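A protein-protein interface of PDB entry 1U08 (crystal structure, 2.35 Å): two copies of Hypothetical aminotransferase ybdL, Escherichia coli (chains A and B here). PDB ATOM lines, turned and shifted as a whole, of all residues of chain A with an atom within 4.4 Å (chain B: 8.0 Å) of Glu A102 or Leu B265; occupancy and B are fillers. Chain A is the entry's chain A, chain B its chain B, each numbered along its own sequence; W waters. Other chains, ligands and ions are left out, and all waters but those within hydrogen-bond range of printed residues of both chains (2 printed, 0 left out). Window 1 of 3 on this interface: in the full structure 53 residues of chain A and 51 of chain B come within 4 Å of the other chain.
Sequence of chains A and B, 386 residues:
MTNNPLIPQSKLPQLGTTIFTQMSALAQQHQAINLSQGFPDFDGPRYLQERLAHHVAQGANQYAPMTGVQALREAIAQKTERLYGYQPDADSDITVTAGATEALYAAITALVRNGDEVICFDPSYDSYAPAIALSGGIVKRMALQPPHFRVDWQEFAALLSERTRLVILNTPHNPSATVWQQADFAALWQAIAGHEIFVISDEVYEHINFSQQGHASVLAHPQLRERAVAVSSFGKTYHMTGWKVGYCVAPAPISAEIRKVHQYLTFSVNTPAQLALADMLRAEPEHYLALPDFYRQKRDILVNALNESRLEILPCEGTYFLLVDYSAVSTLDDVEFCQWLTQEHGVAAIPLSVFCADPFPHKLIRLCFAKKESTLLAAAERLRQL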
ATOM      1  N   THR A  97      14.220   2.666 -21.562  1.00  0.00           N
ATOM      2  CA  THR A  97      12.887   2.702 -22.136  1.00  0.00           C
ATOM      3  C   THR A  97      12.910   3.267 -23.562  1.00  0.00           C
ATOM      4  O   THR A  97      13.885   3.906 -23.962  1.00  0.00           O
ATOM      5  CB  THR A  97      11.982   3.561 -21.243  1.00  0.00           C
ATOM      6  OG1 THR A  97      12.502   4.897 -21.187  1.00  0.00           O
ATOM      7  CG2 THR A  97      11.959   2.994 -19.824  1.00  0.00           C
ATOM      8  N   ALA A  98      11.843   3.036 -24.327  1.00  0.00           N
ATOM      9  CA  ALA A  98      11.777   3.535 -25.703  1.00  0.00           C
ATOM     10  C   ALA A  98      11.464   5.021 -25.693  1.00  0.00           C
ATOM     11  O   ALA A  98      10.375   5.440 -26.097  1.00  0.00           O
ATOM     12  CB  ALA A  98      10.711   2.778 -26.508  1.00  0.00           C
ATOM     13  N   GLY A  99      12.427   5.813 -25.228  1.00  0.00           N
ATOM     14  CA  GLY A  99      12.242   7.252 -25.149  1.00  0.00           C
ATOM     15  C   GLY A  99      11.892   7.665 -23.730  1.00  0.00           C
ATOM     16  O   GLY A  99      11.391   6.848 -22.949  1.00  0.00           O
ATOM     17  N   ALA A 100      12.159   8.921 -23.386  1.00  0.00           N
ATOM     18  CA  ALA A 100      11.852   9.419 -22.050  1.00  0.00           C
ATOM     19  C   ALA A 100      10.349   9.335 -21.851  1.00  0.00           C
ATOM     20  O   ALA A 100       9.866   9.180 -20.726  1.00  0.00           O
ATOM     21  CB  ALA A 100      12.320  10.868 -21.895  1.00  0.00           C
ATOM     22  N   THR A 101       9.616   9.434 -22.958  1.00  0.00           N
ATOM     23  CA  THR A 101       8.161   9.378 -22.930  1.00  0.00           C
ATOM     24  C   THR A 101       7.664   8.093 -22.285  1.00  0.00           C
ATOM     25  O   THR A 101       6.741   8.126 -21.471  1.00  0.00           O
ATOM     26  CB  THR A 101       7.568   9.488 -24.343  1.00  0.00           C
ATOM     27  OG1 THR A 101       7.978  10.725 -24.930  1.00  0.00           O
ATOM     28  CG2 THR A 101       6.046   9.452 -24.292  1.00  0.00           C
ATOM     29  N   GLU A 102       8.267   6.962 -22.641  1.00  0.00           N
ATOM     30  CA  GLU A 102       7.850   5.698 -22.046  1.00  0.00           C
ATOM     31  C   GLU A 102       8.342   5.614 -20.598  1.00  0.00           C
ATOM     32  O   GLU A 102       7.712   4.972 -19.766  1.00  0.00           O
ATOM     33  CB  GLU A 102       8.383   4.483 -22.826  1.00  0.00           C
ATOM     34  CG  GLU A 102       7.762   3.176 -22.315  1.00  0.00           C
ATOM     35  CD  GLU A 102       8.713   1.990 -22.299  1.00  0.00           C
ATOM     36  OE1 GLU A 102       8.503   1.092 -21.461  1.00  0.00           O
ATOM     37  OE2 GLU A 102       9.653   1.937 -23.121  1.00  0.00           O
ATOM     38  N   ALA A 103       9.470   6.248 -20.297  1.00  0.00           N
ATOM     39  CA  ALA A 103       9.980   6.226 -18.931  1.00  0.00           C
ATOM     40  C   ALA A 103       9.011   7.001 -18.032  1.00  0.00           C
ATOM     41  O   ALA A 103       8.788   6.624 -16.885  1.00  0.00           O
ATOM     42  CB  ALA A 103      11.362   6.848 -18.871  1.00  0.00           C
ATOM     43  N   LEU A 104       8.434   8.072 -18.573  1.00  0.00           N
ATOM     44  CA  LEU A 104       7.482   8.902 -17.848  1.00  0.00           C
ATOM     45  C   LEU A 104       6.141   8.189 -17.692  1.00  0.00           C
ATOM     46  O   LEU A 104       5.535   8.228 -16.619  1.00  0.00           O
ATOM     47  CB  LEU A 104       7.273  10.236 -18.570  1.00  0.00           C
ATOM     48  CG  LEU A 104       8.436  11.233 -18.511  1.00  0.00           C
ATOM     49  CD1 LEU A 104       8.223  12.332 -19.562  1.00  0.00           C
ATOM     50  CD2 LEU A 104       8.549  11.826 -17.090  1.00  0.00           C
ATOM     51  N   TYR A 105       5.675   7.538 -18.755  1.00  0.00           N
ATOM     52  CA  TYR A 105       4.407   6.825 -18.685  1.00  0.00           C
ATOM     53  C   TYR A 105       4.516   5.659 -17.699  1.00  0.00           C
ATOM     54  O   TYR A 105       3.607   5.422 -16.900  1.00  0.00           O
ATOM     55  CB  TYR A 105       4.003   6.286 -20.060  1.00  0.00           C
ATOM     56  CG  TYR A 105       2.694   5.536 -20.028  1.00  0.00           C
ATOM     57  CD1 TYR A 105       1.504   6.147 -20.425  1.00  0.00           C
ATOM     58  CD2 TYR A 105       2.634   4.230 -19.535  1.00  0.00           C
ATOM     59  CE1 TYR A 105       0.286   5.475 -20.327  1.00  0.00           C
ATOM     60  CE2 TYR A 105       1.429   3.553 -19.431  1.00  0.00           C
ATOM     61  CZ  TYR A 105       0.263   4.179 -19.827  1.00  0.00           C
ATOM     62  OH  TYR A 105      -0.922   3.496 -19.713  1.00  0.00           O
ATOM     63  N   ALA A 106       5.633   4.940 -17.763  1.00  0.00           N
ATOM     64  CA  ALA A 106       5.869   3.797 -16.891  1.00  0.00           C
ATOM     65  C   ALA A 106       5.966   4.204 -15.429  1.00  0.00           C
ATOM     66  O   ALA A 106       5.356   3.574 -14.562  1.00  0.00           O
ATOM     67  CB  ALA A 106       7.136   3.086 -17.301  1.00  0.00           C
ATOM     68  N   HIS A 262       6.761  -1.300 -17.561  1.00  0.00           N
ATOM     69  CA  HIS A 262       7.538  -1.225 -18.790  1.00  0.00           C
ATOM     70  C   HIS A 262       7.576  -2.554 -19.548  1.00  0.00           C
ATOM     71  O   HIS A 262       7.484  -2.589 -20.779  1.00  0.00           O
ATOM     72  CB  HIS A 262       8.969  -0.788 -18.463  1.00  0.00           C
ATOM     73  CG  HIS A 262       9.975  -1.226 -19.478  1.00  0.00           C
ATOM     74  ND1 HIS A 262       9.967  -0.765 -20.776  1.00  0.00           N
ATOM     75  CD2 HIS A 262      10.981  -2.130 -19.403  1.00  0.00           C
ATOM     76  CE1 HIS A 262      10.923  -1.368 -21.459  1.00  0.00           C
ATOM     77  NE2 HIS A 262      11.552  -2.201 -20.650  1.00  0.00           N
ATOM     78  N   LEU A 265       4.650  -2.966 -21.543  1.00  0.00           N
ATOM     79  CA  LEU A 265       4.451  -1.789 -22.390  1.00  0.00           C
ATOM     80  C   LEU A 265       5.160  -2.020 -23.728  1.00  0.00           C
ATOM     81  O   LEU A 265       4.539  -1.993 -24.787  1.00  0.00           O
ATOM     82  CB  LEU A 265       5.052  -0.552 -21.718  1.00  0.00           C
ATOM     83  CG  LEU A 265       4.156   0.652 -21.438  1.00  0.00           C
ATOM     84  CD1 LEU A 265       3.107   0.293 -20.384  1.00  0.00           C
ATOM     85  CD2 LEU A 265       5.014   1.801 -20.948  1.00  0.00           C
ATOM     86  N   THR A 266       6.470  -2.245 -23.653  1.00  0.00           N
ATOM     87  CA  THR A 266       7.312  -2.491 -24.824  1.00  0.00           C
ATOM     88  C   THR A 266       8.223  -3.701 -24.571  1.00  0.00           C
ATOM     89  O   THR A 266       8.791  -4.278 -25.496  1.00  0.00           O
ATOM     90  CB  THR A 266       8.209  -1.259 -25.125  1.00  0.00           C
ATOM     91  OG1 THR A 266       8.938  -0.907 -23.940  1.00  0.00           O
ATOM     92  CG2 THR A 266       7.365  -0.065 -25.562  1.00  0.00           C
ATOM     93  N   THR B  97       3.812   0.949 -33.891  1.00  0.00           N
ATOM     94  CA  THR B  97       4.125   0.921 -32.466  1.00  0.00           C
ATOM     95  C   THR B  97       5.500   0.308 -32.208  1.00  0.00           C
ATOM     96  O   THR B  97       6.031  -0.416 -33.051  1.00  0.00           O
ATOM     97  CB  THR B  97       3.084   0.097 -31.697  1.00  0.00           C
ATOM     98  OG1 THR B  97       3.112  -1.257 -32.179  1.00  0.00           O
ATOM     99  CG2 THR B  97       1.673   0.680 -31.899  1.00  0.00           C
ATOM    100  N   ALA B  98       6.067   0.595 -31.039  1.00  0.00           N
ATOM    101  CA  ALA B  98       7.377   0.073 -30.670  1.00  0.00           C
ATOM    102  C   ALA B  98       7.283  -1.411 -30.338  1.00  0.00           C
ATOM    103  O   ALA B  98       7.496  -1.814 -29.202  1.00  0.00           O
ATOM    104  CB  ALA B  98       7.918   0.843 -29.480  1.00  0.00           C
ATOM    105  N   THR B 101       4.151  -5.732 -28.851  1.00  0.00           N
ATOM    106  CA  THR B 101       3.897  -5.618 -27.416  1.00  0.00           C
ATOM    107  C   THR B 101       3.181  -4.302 -27.097  1.00  0.00           C
ATOM    108  O   THR B 101       2.167  -4.306 -26.404  1.00  0.00           O
ATOM    109  CB  THR B 101       5.215  -5.681 -26.594  1.00  0.00           C
ATOM    110  OG1 THR B 101       5.938  -6.873 -26.920  1.00  0.00           O
ATOM    111  CG2 THR B 101       4.914  -5.693 -25.103  1.00  0.00           C
ATOM    112  N   GLU B 102       3.698  -3.183 -27.598  1.00  0.00           N
ATOM    113  CA  GLU B 102       3.059  -1.884 -27.353  1.00  0.00           C
ATOM    114  C   GLU B 102       1.680  -1.757 -28.014  1.00  0.00           C
ATOM    115  O   GLU B 102       0.810  -1.062 -27.497  1.00  0.00           O
ATOM    116  CB  GLU B 102       3.933  -0.715 -27.846  1.00  0.00           C
ATOM    117  CG  GLU B 102       3.401   0.635 -27.352  1.00  0.00           C
ATOM    118  CD  GLU B 102       3.581   1.777 -28.338  1.00  0.00           C
ATOM    119  OE1 GLU B 102       2.914   2.818 -28.156  1.00  0.00           O
ATOM    120  OE2 GLU B 102       4.386   1.653 -29.283  1.00  0.00           O
ATOM    121  N   ALA B 103       1.489  -2.400 -29.166  1.00  0.00           N
ATOM    122  CA  ALA B 103       0.203  -2.336 -29.862  1.00  0.00           C
ATOM    123  C   ALA B 103      -0.841  -3.043 -29.013  1.00  0.00           C
ATOM    124  O   ALA B 103      -1.983  -2.587 -28.899  1.00  0.00           O
ATOM    125  CB  ALA B 103       0.299  -3.008 -31.222  1.00  0.00           C
ATOM    126  N   LEU B 104      -0.438  -4.163 -28.417  1.00  0.00           N
ATOM    127  CA  LEU B 104      -1.333  -4.941 -27.574  1.00  0.00           C
ATOM    128  C   LEU B 104      -1.687  -4.134 -26.324  1.00  0.00           C
ATOM    129  O   LEU B 104      -2.858  -4.046 -25.954  1.00  0.00           O
ATOM    130  CB  LEU B 104      -0.672  -6.271 -27.189  1.00  0.00           C
ATOM    131  CG  LEU B 104      -0.477  -7.257 -28.352  1.00  0.00           C
ATOM    132  CD1 LEU B 104       0.498  -8.339 -27.968  1.00  0.00           C
ATOM    133  CD2 LEU B 104      -1.808  -7.875 -28.729  1.00  0.00           C
ATOM    134  N   TYR B 105      -0.680  -3.542 -25.680  1.00  0.00           N
ATOM    135  CA  TYR B 105      -0.914  -2.739 -24.485  1.00  0.00           C
ATOM    136  C   TYR B 105      -1.761  -1.510 -24.820  1.00  0.00           C
ATOM    137  O   TYR B 105      -2.625  -1.120 -24.043  1.00  0.00           O
ATOM    138  CB  TYR B 105       0.417  -2.296 -23.854  1.00  0.00           C
ATOM    139  CG  TYR B 105       0.233  -1.477 -22.592  1.00  0.00           C
ATOM    140  CD1 TYR B 105       0.336  -2.062 -21.327  1.00  0.00           C
ATOM    141  CD2 TYR B 105      -0.110  -0.129 -22.666  1.00  0.00           C
ATOM    142  CE1 TYR B 105       0.097  -1.317 -20.168  1.00  0.00           C
ATOM    143  CE2 TYR B 105      -0.354   0.619 -21.529  1.00  0.00           C
ATOM    144  CZ  TYR B 105      -0.251   0.026 -20.284  1.00  0.00           C
ATOM    145  OH  TYR B 105      -0.503   0.781 -19.162  1.00  0.00           O
ATOM    146  N   ALA B 106      -1.525  -0.900 -25.977  1.00  0.00           N
ATOM    147  CA  ALA B 106      -2.298   0.280 -26.363  1.00  0.00           C
ATOM    148  C   ALA B 106      -3.739  -0.083 -26.699  1.00  0.00           C
ATOM    149  O   ALA B 106      -4.673   0.604 -26.274  1.00  0.00           O
ATOM    150  CB  ALA B 106      -1.654   0.971 -27.547  1.00  0.00           C
ATOM    151  N   ALA B 107      -3.922  -1.158 -27.464  1.00  0.00           N
ATOM    152  CA  ALA B 107      -5.265  -1.597 -27.843  1.00  0.00           C
ATOM    153  C   ALA B 107      -6.064  -2.006 -26.609  1.00  0.00           C
ATOM    154  O   ALA B 107      -7.222  -1.620 -26.455  1.00  0.00           O
ATOM    155  CB  ALA B 107      -5.187  -2.764 -28.826  1.00  0.00           C
ATOM    156  N   THR B 109      -5.492  -1.145 -23.446  1.00  0.00           N
ATOM    157  CA  THR B 109      -5.705   0.033 -22.618  1.00  0.00           C
ATOM    158  C   THR B 109      -6.769   0.966 -23.181  1.00  0.00           C
ATOM    159  O   THR B 109      -7.518   1.575 -22.428  1.00  0.00           O
ATOM    160  CB  THR B 109      -4.398   0.807 -22.439  1.00  0.00           C
ATOM    161  OG1 THR B 109      -3.428  -0.054 -21.829  1.00  0.00           O
ATOM    162  CG2 THR B 109      -4.616   2.041 -21.562  1.00  0.00           C
ATOM    163  N   ILE B 258      -6.739   3.937 -29.974  1.00  0.00           N
ATOM    164  CA  ILE B 258      -5.482   3.251 -29.750  1.00  0.00           C
ATOM    165  C   ILE B 258      -4.386   4.323 -29.809  1.00  0.00           C
ATOM    166  O   ILE B 258      -3.445   4.329 -29.012  1.00  0.00           O
ATOM    167  CB  ILE B 258      -5.238   2.192 -30.833  1.00  0.00           C
ATOM    168  CG1 ILE B 258      -6.258   1.054 -30.685  1.00  0.00           C
ATOM    169  CG2 ILE B 258      -3.813   1.687 -30.749  1.00  0.00           C
ATOM    170  CD1 ILE B 258      -6.183  -0.005 -31.783  1.00  0.00           C
ATOM    171  N   ARG B 259      -4.535   5.250 -30.749  1.00  0.00           N
ATOM    172  CA  ARG B 259      -3.565   6.322 -30.923  1.00  0.00           C
ATOM    173  C   ARG B 259      -3.526   7.275 -29.733  1.00  0.00           C
ATOM    174  O   ARG B 259      -2.457   7.736 -29.353  1.00  0.00           O
ATOM    175  CB  ARG B 259      -3.866   7.090 -32.212  1.00  0.00           C
ATOM    176  CG  ARG B 259      -3.623   6.263 -33.465  1.00  0.00           C
ATOM    177  CD  ARG B 259      -4.257   6.880 -34.692  1.00  0.00           C
ATOM    178  NE  ARG B 259      -3.813   6.212 -35.910  1.00  0.00           N
ATOM    179  CZ  ARG B 259      -4.058   6.669 -37.131  1.00  0.00           C
ATOM    180  NH1 ARG B 259      -4.746   7.789 -37.282  1.00  0.00           N
ATOM    181  NH2 ARG B 259      -3.592   6.027 -38.194  1.00  0.00           N
ATOM    182  N   LYS B 260      -4.678   7.567 -29.138  1.00  0.00           N
ATOM    183  CA  LYS B 260      -4.690   8.469 -27.990  1.00  0.00           C
ATOM    184  C   LYS B 260      -3.808   7.915 -26.887  1.00  0.00           C
ATOM    185  O   LYS B 260      -3.100   8.671 -26.241  1.00  0.00           O
ATOM    186  CB  LYS B 260      -6.111   8.697 -27.470  1.00  0.00           C
ATOM    187  CG  LYS B 260      -6.940   9.622 -28.351  1.00  0.00           C
ATOM    188  CD  LYS B 260      -8.316   9.902 -27.745  1.00  0.00           C
ATOM    189  CE  LYS B 260      -9.212  10.644 -28.728  1.00  0.00           C
ATOM    190  NZ  LYS B 260     -10.618  10.755 -28.242  1.00  0.00           N
ATOM    191  N   VAL B 261      -3.837   6.598 -26.683  1.00  0.00           N
ATOM    192  CA  VAL B 261      -3.010   5.966 -25.655  1.00  0.00           C
ATOM    193  C   VAL B 261      -1.556   5.927 -26.107  1.00  0.00           C
ATOM    194  O   VAL B 261      -0.669   6.385 -25.388  1.00  0.00           O
ATOM    195  CB  VAL B 261      -3.465   4.519 -25.340  1.00  0.00           C
ATOM    196  CG1 VAL B 261      -2.440   3.835 -24.445  1.00  0.00           C
ATOM    197  CG2 VAL B 261      -4.815   4.533 -24.649  1.00  0.00           C
ATOM    198  N   HIS B 262      -1.325   5.382 -27.304  1.00  0.00           N
ATOM    199  CA  HIS B 262       0.014   5.280 -27.884  1.00  0.00           C
ATOM    200  C   HIS B 262       0.809   6.587 -27.795  1.00  0.00           C
ATOM    201  O   HIS B 262       1.955   6.611 -27.350  1.00  0.00           O
ATOM    202  CB  HIS B 262      -0.094   4.855 -29.358  1.00  0.00           C
ATOM    203  CG  HIS B 262       1.121   5.180 -30.175  1.00  0.00           C
ATOM    204  ND1 HIS B 262       2.331   4.540 -30.000  1.00  0.00           N
ATOM    205  CD2 HIS B 262       1.322   6.103 -31.146  1.00  0.00           C
ATOM    206  CE1 HIS B 262       3.222   5.056 -30.828  1.00  0.00           C
ATOM    207  NE2 HIS B 262       2.637   6.006 -31.535  1.00  0.00           N
ATOM    208  N   GLN B 263       0.188   7.672 -28.236  1.00  0.00           N
ATOM    209  CA  GLN B 263       0.816   8.980 -28.245  1.00  0.00           C
ATOM    210  C   GLN B 263       1.470   9.407 -26.928  1.00  0.00           C
ATOM    211  O   GLN B 263       2.421  10.197 -26.935  1.00  0.00           O
ATOM    212  CB  GLN B 263      -0.215  10.004 -28.732  1.00  0.00           C
ATOM    213  CG  GLN B 263      -0.301  11.288 -27.969  1.00  0.00           C
ATOM    214  CD  GLN B 263      -1.148  12.305 -28.705  1.00  0.00           C
ATOM    215  OE1 GLN B 263      -2.267  12.003 -29.136  1.00  0.00           O
ATOM    216  NE2 GLN B 263      -0.619  13.521 -28.859  1.00  0.00           N
ATOM    217  N   TYR B 264       0.989   8.878 -25.804  1.00  0.00           N
ATOM    218  CA  TYR B 264       1.570   9.215 -24.506  1.00  0.00           C
ATOM    219  C   TYR B 264       2.362   8.037 -23.942  1.00  0.00           C
ATOM    220  O   TYR B 264       2.930   8.115 -22.846  1.00  0.00           O
ATOM    221  CB  TYR B 264       0.475   9.647 -23.527  1.00  0.00           C
ATOM    222  CG  TYR B 264      -0.328  10.824 -24.030  1.00  0.00           C
ATOM    223  CD1 TYR B 264       0.270  12.066 -24.232  1.00  0.00           C
ATOM    224  CD2 TYR B 264      -1.680  10.681 -24.357  1.00  0.00           C
ATOM    225  CE1 TYR B 264      -0.455  13.141 -24.758  1.00  0.00           C
ATOM    226  CE2 TYR B 264      -2.412  11.749 -24.884  1.00  0.00           C
ATOM    227  CZ  TYR B 264      -1.790  12.974 -25.085  1.00  0.00           C
ATOM    228  OH  TYR B 264      -2.489  14.017 -25.652  1.00  0.00           O
ATOM    229  N   LEU B 265       2.401   6.948 -24.703  1.00  0.00           N
ATOM    230  CA  LEU B 265       3.139   5.750 -24.306  1.00  0.00           C
ATOM    231  C   LEU B 265       4.574   5.887 -24.806  1.00  0.00           C
ATOM    232  O   LEU B 265       5.536   5.713 -24.057  1.00  0.00           O
ATOM    233  CB  LEU B 265       2.507   4.504 -24.939  1.00  0.00           C
ATOM    234  CG  LEU B 265       1.920   3.368 -24.093  1.00  0.00           C
ATOM    235  CD1 LEU B 265       0.774   3.882 -23.232  1.00  0.00           C
ATOM    236  CD2 LEU B 265       1.419   2.258 -25.021  1.00  0.00           C
ATOM    237  N   THR B 266       4.708   6.206 -26.089  1.00  0.00           N
ATOM    238  CA  THR B 266       6.015   6.355 -26.709  1.00  0.00           C
ATOM    239  C   THR B 266       6.019   7.528 -27.690  1.00  0.00           C
ATOM    240  O   THR B 266       7.075   8.018 -28.084  1.00  0.00           O
ATOM    241  CB  THR B 266       6.396   5.050 -27.455  1.00  0.00           C
ATOM    242  OG1 THR B 266       5.341   4.698 -28.362  1.00  0.00           O
ATOM    243  CG2 THR B 266       6.594   3.890 -26.463  1.00  0.00           C
ATOM    244  N   PHE B 267       4.816   7.971 -28.054  1.00  0.00           N
ATOM    245  CA  PHE B 267       4.569   9.061 -29.003  1.00  0.00           C
ATOM    246  C   PHE B 267       4.872   8.675 -30.441  1.00  0.00           C
ATOM    247  O   PHE B 267       3.987   8.702 -31.298  1.00  0.00           O
ATOM    248  CB  PHE B 267       5.365  10.323 -28.683  1.00  0.00           C
ATOM    249  CG  PHE B 267       5.095  11.440 -29.649  1.00  0.00           C
ATOM    250  CD1 PHE B 267       3.884  12.132 -29.609  1.00  0.00           C
ATOM    251  CD2 PHE B 267       6.017  11.756 -30.646  1.00  0.00           C
ATOM    252  CE1 PHE B 267       3.591  13.124 -30.548  1.00  0.00           C
ATOM    253  CE2 PHE B 267       5.734  12.744 -31.589  1.00  0.00           C
ATOM    254  CZ  PHE B 267       4.513  13.430 -31.539  1.00  0.00           C
ATOM    255  N   SER B 268       6.133   8.350 -30.712  1.00  0.00           N
ATOM    256  CA  SER B 268       6.542   7.940 -32.049  1.00  0.00           C
ATOM    257  C   SER B 268       7.458   6.739 -31.908  1.00  0.00           C
ATOM    258  O   SER B 268       7.891   6.393 -30.803  1.00  0.00           O
ATOM    259  CB  SER B 268       7.265   9.068 -32.784  1.00  0.00           C
ATOM    260  OG  SER B 268       8.445   9.444 -32.096  1.00  0.00           O
HETATM  261  O   HOH W   1       9.469   4.404 -29.178  1.00  0.00           O
HETATM  262  O   HOH W   2       4.665  10.018 -21.065  1.00  0.00           O
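The side-chain hydroxyl of Tyr B105 is in hydrogen-bond range of the side-chain hydroxyl of Tyr A105 (2.8 Å).
The backbone NH of Glu A102 sits close to the backbone carbonyl oxygen of Leu B265, at 3.3 Å.
The backbone carbonyl oxygen (O) of Leu A265 sits close to the backbone NH (N) of Glu B102, at 3.2 Å.
OE1 of Glu B102 sits at hydrogen-bond distance from ND1 of His B262 (2.6 Å).
N of Ala A98 sits at hydrogen-bond distance from OE2 of Glu A102 (2.7 Å).
OE1 of Glu A102 is in hydrogen-bond range of ND1 of His A262 (2.5 Å).
The backbone carbonyl oxygen (O) of Tyr B105 sits at hydrogen-bond distance from the side-chain hydroxyl (OG1) of Thr B109, at 2.6 Å.
OE2 of Glu A102 lies within hydrogen-bond range of OG1 of Thr A266, 3.0 Å away.
OG1 of Thr A266 sits close to ND1 of His A262 (3.3 Å).
Thr A101 touches Leu B265, and with the chains exchanged Leu A265 touches Thr B101.
Thr A101 touches Thr B266, and with the chains exchanged Thr A266 touches Thr B101.
Glu A102 touches Leu B265, and with the chains exchanged Leu A265 touches Glu B102.
Tyr A105 touches its own counterpart, Tyr B105.
Of the 21 printed residues of chain B, 6 touch a printed residue of chain A.
Along chain B the printed residues that touch a printed residue of chain A span positions 101 to 266.
Water W2 bridges O of Thr A101 (2.8 Å) and O of Tyr B264 (3.1 Å).
Water W1 lies within hydrogen-bond range of the backbone carbonyl oxygen (O) of Ser B268 and the backbone carbonyl oxygen (O) of Ala A98.
Glu A102 touches just one residue of chain B: Leu B265 (3.1 Å).
Of chain A, only Thr A101, Glu A102 and Tyr A105 come within 4 Å of Leu B265.
Ala A103 touches none of the printed residues of chain B.
Of the printed residues of chain A, Tyr B105 touches Tyr A105 and Leu A265.
Printed residues of chain A within 4 Å of Glu B102: Leu A265.
Printed residues of chain B within 4 Å of Tyr A105: Tyr B105, Tyr B264 and Leu B265.
The nearest residue of chain B that does not touch Glu A102 is Thr B266 (4.1 Å).
Thr A101 touches Tyr B264 (CG2 to O, 3.7 Å).
Thr A101 touches Leu B265.
Thr A101 touches Thr B266 (CG2 to C, 3.9 Å).
CD1 of Tyr A105 touches O of Tyr B264 (3.4 Å).
Tyr A105 touches Leu B265.
C of Thr B101 touches O of Leu A265 (3.5 Å).
Tyr B105 touches Leu A265 (CZ to CD1, 3.4 Å).
C of Thr A266 touches CG2 of Thr B101, at 3.9 Å.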
